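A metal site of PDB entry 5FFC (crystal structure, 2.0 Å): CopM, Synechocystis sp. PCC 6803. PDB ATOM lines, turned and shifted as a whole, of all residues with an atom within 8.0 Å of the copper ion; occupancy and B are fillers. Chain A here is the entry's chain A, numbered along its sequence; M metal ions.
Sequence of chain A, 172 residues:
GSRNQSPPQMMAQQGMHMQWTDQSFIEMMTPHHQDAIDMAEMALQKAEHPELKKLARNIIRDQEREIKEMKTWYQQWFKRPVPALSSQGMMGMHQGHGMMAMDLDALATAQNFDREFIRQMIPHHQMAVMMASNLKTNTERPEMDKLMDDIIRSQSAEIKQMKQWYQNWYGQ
The copper ion is bound by OD2 of Asp 35, at 1.8 Å. ND1 of His 32 binds the copper ion (1.9 Å). The copper ion is bound by NE2 of His 124 (2.2 Å). Slightly farther from the copper ion lies OD1 of Asp 35 (2.8 Å).
Within 4 Å of the copper ion: His 32, Asp 35 and His 124. The nearest printed residue that does not touch the copper ion is Met 100 (4.3 Å).
SD of Met 127 lies close to NE2 of His 32 (3.8 Å). NE2 of His 32 lies within hydrogen-bond range of O of Met 99, 2.8 Å away.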
ATOM      1  N   MET A  28     -26.037  -4.760  32.874  1.00  0.00           N
ATOM      2  CA  MET A  28     -24.968  -4.542  31.921  1.00  0.00           C
ATOM      3  C   MET A  28     -25.500  -4.154  30.537  1.00  0.00           C
ATOM      4  O   MET A  28     -24.917  -3.313  29.854  1.00  0.00           O
ATOM      5  CB  MET A  28     -24.098  -5.796  31.803  1.00  0.00           C
ATOM      6  N   MET A  29     -26.602  -4.783  30.144  1.00  0.00           N
ATOM      7  CA  MET A  29     -27.134  -4.594  28.792  1.00  0.00           C
ATOM      8  C   MET A  29     -27.774  -3.245  28.538  1.00  0.00           C
ATOM      9  O   MET A  29     -27.708  -2.721  27.430  1.00  0.00           O
ATOM     10  CB  MET A  29     -28.075  -5.724  28.415  1.00  0.00           C
ATOM     11  CG  MET A  29     -27.325  -6.969  27.991  1.00  0.00           C
ATOM     12  SD  MET A  29     -26.182  -6.594  26.636  1.00  0.00           S
ATOM     13  CE  MET A  29     -27.346  -6.180  25.352  1.00  0.00           C
ATOM     14  N   THR A  30     -28.397  -2.686  29.574  1.00  0.00           N
ATOM     15  CA  THR A  30     -29.003  -1.358  29.464  1.00  0.00           C
ATOM     16  C   THR A  30     -27.999  -0.273  29.034  1.00  0.00           C
ATOM     17  O   THR A  30     -28.254   0.429  28.053  1.00  0.00           O
ATOM     18  CB  THR A  30     -29.769  -0.976  30.758  1.00  0.00           C
ATOM     19  OG1 THR A  30     -30.660  -2.038  31.125  1.00  0.00           O
ATOM     20  CG2 THR A  30     -30.564   0.311  30.539  1.00  0.00           C
ATOM     21  N   PRO A  31     -26.866  -0.131  29.747  1.00  0.00           N
ATOM     22  CA  PRO A  31     -25.876   0.843  29.269  1.00  0.00           C
ATOM     23  C   PRO A  31     -25.320   0.483  27.897  1.00  0.00           C
ATOM     24  O   PRO A  31     -25.035   1.377  27.101  1.00  0.00           O
ATOM     25  CB  PRO A  31     -24.750   0.750  30.312  1.00  0.00           C
ATOM     26  CG  PRO A  31     -25.388   0.156  31.521  1.00  0.00           C
ATOM     27  CD  PRO A  31     -26.417  -0.784  30.989  1.00  0.00           C
ATOM     28  N   HIS A  32     -25.153  -0.815  27.637  1.00  0.00           N
ATOM     29  CA  HIS A  32     -24.635  -1.267  26.349  1.00  0.00           C
ATOM     30  C   HIS A  32     -25.565  -0.937  25.177  1.00  0.00           C
ATOM     31  O   HIS A  32     -25.104  -0.636  24.081  1.00  0.00           O
ATOM     32  CB  HIS A  32     -24.326  -2.761  26.369  1.00  0.00           C
ATOM     33  CG  HIS A  32     -22.880  -3.068  26.568  1.00  0.00           C
ATOM     34  ND1 HIS A  32     -21.888  -2.435  25.850  1.00  0.00           N
ATOM     35  CD2 HIS A  32     -22.250  -3.949  27.386  1.00  0.00           C
ATOM     36  CE1 HIS A  32     -20.711  -2.899  26.222  1.00  0.00           C
ATOM     37  NE2 HIS A  32     -20.900  -3.827  27.153  1.00  0.00           N
ATOM     38  N   HIS A  33     -26.871  -1.023  25.401  1.00  0.00           N
ATOM     39  CA  HIS A  33     -27.842  -0.671  24.364  1.00  0.00           C
ATOM     40  C   HIS A  33     -27.790   0.826  24.087  1.00  0.00           C
ATOM     41  O   HIS A  33     -28.172   1.267  23.004  1.00  0.00           O
ATOM     42  CB  HIS A  33     -29.264  -1.096  24.749  1.00  0.00           C
ATOM     43  CG  HIS A  33     -29.675  -2.439  24.206  1.00  0.00           C
ATOM     44  ND1 HIS A  33     -28.762  -3.429  23.889  1.00  0.00           N
ATOM     45  CD2 HIS A  33     -30.893  -2.944  23.930  1.00  0.00           C
ATOM     46  CE1 HIS A  33     -29.406  -4.487  23.436  1.00  0.00           C
ATOM     47  NE2 HIS A  33     -30.707  -4.226  23.454  1.00  0.00           N
ATOM     48  N   GLN A  34     -27.310   1.603  25.045  1.00  0.00           N
ATOM     49  CA  GLN A  34     -27.280   3.054  24.894  1.00  0.00           C
ATOM     50  C   GLN A  34     -26.233   3.540  23.905  1.00  0.00           C
ATOM     51  O   GLN A  34     -26.539   4.364  23.039  1.00  0.00           O
ATOM     52  CB  GLN A  34     -27.072   3.747  26.243  1.00  0.00           C
ATOM     53  CG  GLN A  34     -27.129   5.278  26.155  1.00  0.00           C
ATOM     54  CD  GLN A  34     -28.434   5.775  25.568  1.00  0.00           C
ATOM     55  OE1 GLN A  34     -28.446   6.618  24.674  1.00  0.00           O
ATOM     56  NE2 GLN A  34     -29.550   5.255  26.075  1.00  0.00           N
ATOM     57  N   ASP A  35     -25.006   3.054  24.037  1.00  0.00           N
ATOM     58  CA  ASP A  35     -23.930   3.479  23.147  1.00  0.00           C
ATOM     59  C   ASP A  35     -24.269   3.150  21.685  1.00  0.00           C
ATOM     60  O   ASP A  35     -23.946   3.914  20.777  1.00  0.00           O
ATOM     61  CB  ASP A  35     -22.577   2.889  23.570  1.00  0.00           C
ATOM     62  CG  ASP A  35     -22.587   1.364  23.624  1.00  0.00           C
ATOM     63  OD1 ASP A  35     -23.211   0.736  22.754  1.00  0.00           O
ATOM     64  OD2 ASP A  35     -21.943   0.792  24.531  1.00  0.00           O
ATOM     65  N   ALA A  36     -24.920   2.008  21.484  1.00  0.00           N
ATOM     66  CA  ALA A  36     -25.367   1.612  20.154  1.00  0.00           C
ATOM     67  C   ALA A  36     -26.353   2.629  19.587  1.00  0.00           C
ATOM     68  O   ALA A  36     -26.216   3.059  18.448  1.00  0.00           O
ATOM     69  CB  ALA A  36     -26.012   0.244  20.208  1.00  0.00           C
ATOM     70  N   ILE A  37     -27.323   3.008  20.413  1.00  0.00           N
ATOM     71  CA  ILE A  37     -28.326   3.993  20.030  1.00  0.00           C
ATOM     72  C   ILE A  37     -27.665   5.311  19.619  1.00  0.00           C
ATOM     73  O   ILE A  37     -28.026   5.888  18.598  1.00  0.00           O
ATOM     74  CB  ILE A  37     -29.369   4.213  21.149  1.00  0.00           C
ATOM     75  CG1 ILE A  37     -30.279   2.995  21.263  1.00  0.00           C
ATOM     76  CG2 ILE A  37     -30.205   5.465  20.879  1.00  0.00           C
ATOM     77  CD1 ILE A  37     -31.277   3.064  22.398  1.00  0.00           C
ATOM     78  N   GLN A  63     -33.634  -1.383  19.919  1.00  0.00           N
ATOM     79  CA  GLN A  63     -32.877  -1.356  21.149  1.00  0.00           C
ATOM     80  C   GLN A  63     -33.498  -0.459  22.205  1.00  0.00           C
ATOM     81  O   GLN A  63     -33.401  -0.725  23.398  1.00  0.00           O
ATOM     82  CB  GLN A  63     -31.393  -1.078  20.863  1.00  0.00           C
ATOM     83  CG  GLN A  63     -30.803  -2.140  19.935  1.00  0.00           C
ATOM     84  CD  GLN A  63     -29.309  -2.330  20.115  1.00  0.00           C
ATOM     85  OE1 GLN A  63     -28.732  -1.935  21.135  1.00  0.00           O
ATOM     86  NE2 GLN A  63     -28.659  -2.940  19.120  1.00  0.00           N
ATOM     87  N   MET A  93     -19.692   4.210  30.892  1.00  0.00           N
ATOM     88  CA  MET A  93     -19.367   3.297  29.791  1.00  0.00           C
ATOM     89  C   MET A  93     -18.429   3.938  28.766  1.00  0.00           C
ATOM     90  O   MET A  93     -18.804   4.867  28.070  1.00  0.00           O
ATOM     91  CB  MET A  93     -20.641   2.845  29.079  1.00  0.00           C
ATOM     92  CG  MET A  93     -21.129   1.466  29.494  1.00  0.00           C
ATOM     93  SD  MET A  93     -20.036   0.138  28.973  1.00  0.00           S
ATOM     94  CE  MET A  93     -21.110  -1.272  29.254  1.00  0.00           C
ATOM     95  N   HIS A  94     -17.214   3.407  28.687  1.00  0.00           N
ATOM     96  CA  HIS A  94     -16.205   3.928  27.768  1.00  0.00           C
ATOM     97  C   HIS A  94     -15.022   2.964  27.670  1.00  0.00           C
ATOM     98  O   HIS A  94     -14.855   2.085  28.508  1.00  0.00           O
ATOM     99  CB  HIS A  94     -15.728   5.314  28.195  1.00  0.00           C
ATOM    100  CG  HIS A  94     -15.285   5.395  29.623  1.00  0.00           C
ATOM    101  ND1 HIS A  94     -16.127   5.147  30.685  1.00  0.00           N
ATOM    102  CD2 HIS A  94     -14.084   5.705  30.169  1.00  0.00           C
ATOM    103  CE1 HIS A  94     -15.470   5.289  31.815  1.00  0.00           C
ATOM    104  NE2 HIS A  94     -14.230   5.638  31.529  1.00  0.00           N
ATOM    105  N   MET A  99     -14.934  -3.293  28.829  1.00  0.00           N
ATOM    106  CA  MET A  99     -16.390  -3.334  28.772  1.00  0.00           C
ATOM    107  C   MET A  99     -16.881  -3.540  27.334  1.00  0.00           C
ATOM    108  O   MET A  99     -18.070  -3.720  27.100  1.00  0.00           O
ATOM    109  CB  MET A  99     -17.006  -2.062  29.354  1.00  0.00           C
ATOM    110  CG  MET A  99     -16.713  -1.851  30.834  1.00  0.00           C
ATOM    111  SD  MET A  99     -17.534  -3.054  31.898  1.00  0.00           S
ATOM    112  CE  MET A  99     -19.139  -2.278  32.111  1.00  0.00           C
ATOM    113  N   MET A 100     -15.942  -3.503  26.387  1.00  0.00           N
ATOM    114  CA  MET A 100     -16.229  -3.584  24.957  1.00  0.00           C
ATOM    115  C   MET A 100     -17.123  -2.430  24.514  1.00  0.00           C
ATOM    116  O   MET A 100     -18.037  -2.616  23.715  1.00  0.00           O
ATOM    117  CB  MET A 100     -16.823  -4.934  24.569  1.00  0.00           C
ATOM    118  CG  MET A 100     -16.056  -6.127  25.122  1.00  0.00           C
ATOM    119  SD  MET A 100     -16.630  -7.716  24.487  1.00  0.00           S
ATOM    120  CE  MET A 100     -15.696  -7.835  22.963  1.00  0.00           C
ATOM    121  N   ALA A 101     -16.846  -1.230  25.030  1.00  0.00           N
ATOM    122  CA  ALA A 101     -17.607  -0.047  24.672  1.00  0.00           C
ATOM    123  C   ALA A 101     -17.124   0.513  23.339  1.00  0.00           C
ATOM    124  O   ALA A 101     -16.095   0.098  22.810  1.00  0.00           O
ATOM    125  CB  ALA A 101     -17.490   1.011  25.760  1.00  0.00           C
ATOM    126  N   MET A 102     -17.869   1.476  22.803  1.00  0.00           N
ATOM    127  CA  MET A 102     -17.546   2.073  21.511  1.00  0.00           C
ATOM    128  C   MET A 102     -16.981   3.488  21.656  1.00  0.00           C
ATOM    129  O   MET A 102     -16.941   4.054  22.747  1.00  0.00           O
ATOM    130  CB  MET A 102     -18.764   2.019  20.584  1.00  0.00           C
ATOM    131  CG  MET A 102     -19.136   0.580  20.237  1.00  0.00           C
ATOM    132  SD  MET A 102     -20.424   0.391  18.990  1.00  0.00           S
ATOM    133  CE  MET A 102     -21.858   0.951  19.907  1.00  0.00           C
ATOM    134  N   HIS A 124     -19.604  -5.019  18.568  1.00  0.00           N
ATOM    135  CA  HIS A 124     -20.600  -4.642  19.576  1.00  0.00           C
ATOM    136  C   HIS A 124     -21.848  -5.510  19.460  1.00  0.00           C
ATOM    137  O   HIS A 124     -22.412  -5.939  20.478  1.00  0.00           O
ATOM    138  CB  HIS A 124     -20.960  -3.167  19.458  1.00  0.00           C
ATOM    139  CG  HIS A 124     -21.720  -2.634  20.628  1.00  0.00           C
ATOM    140  ND1 HIS A 124     -23.094  -2.649  20.713  1.00  0.00           N
ATOM    141  CD2 HIS A 124     -21.290  -2.078  21.789  1.00  0.00           C
ATOM    142  CE1 HIS A 124     -23.484  -2.128  21.856  1.00  0.00           C
ATOM    143  NE2 HIS A 124     -22.405  -1.768  22.531  1.00  0.00           N
ATOM    144  N   HIS A 125     -22.288  -5.762  18.225  1.00  0.00           N
ATOM    145  CA  HIS A 125     -23.414  -6.672  17.995  1.00  0.00           C
ATOM    146  C   HIS A 125     -23.078  -8.111  18.399  1.00  0.00           C
ATOM    147  O   HIS A 125     -23.888  -8.796  19.032  1.00  0.00           O
ATOM    148  CB  HIS A 125     -23.846  -6.625  16.522  1.00  0.00           C
ATOM    149  CG  HIS A 125     -24.960  -5.669  16.237  1.00  0.00           C
ATOM    150  ND1 HIS A 125     -25.043  -4.424  16.824  1.00  0.00           N
ATOM    151  CD2 HIS A 125     -26.026  -5.767  15.408  1.00  0.00           C
ATOM    152  CE1 HIS A 125     -26.122  -3.806  16.378  1.00  0.00           C
ATOM    153  NE2 HIS A 125     -26.745  -4.595  15.521  1.00  0.00           N
ATOM    154  N   MET A 127     -20.994  -9.078  20.625  1.00  0.00           N
ATOM    155  CA  MET A 127     -21.007  -9.096  22.080  1.00  0.00           C
ATOM    156  C   MET A 127     -22.420  -9.321  22.635  1.00  0.00           C
ATOM    157  O   MET A 127     -22.606 -10.149  23.528  1.00  0.00           O
ATOM    158  CB  MET A 127     -20.433  -7.785  22.624  1.00  0.00           C
ATOM    159  CG  MET A 127     -20.329  -7.709  24.136  1.00  0.00           C
ATOM    160  SD  MET A 127     -21.636  -6.696  24.851  1.00  0.00           S
ATOM    161  CE  MET A 127     -21.574  -5.252  23.794  1.00  0.00           C
HETATM  162 CU    CU M   1     -21.927  -1.020  24.553  1.00  0.00          CU
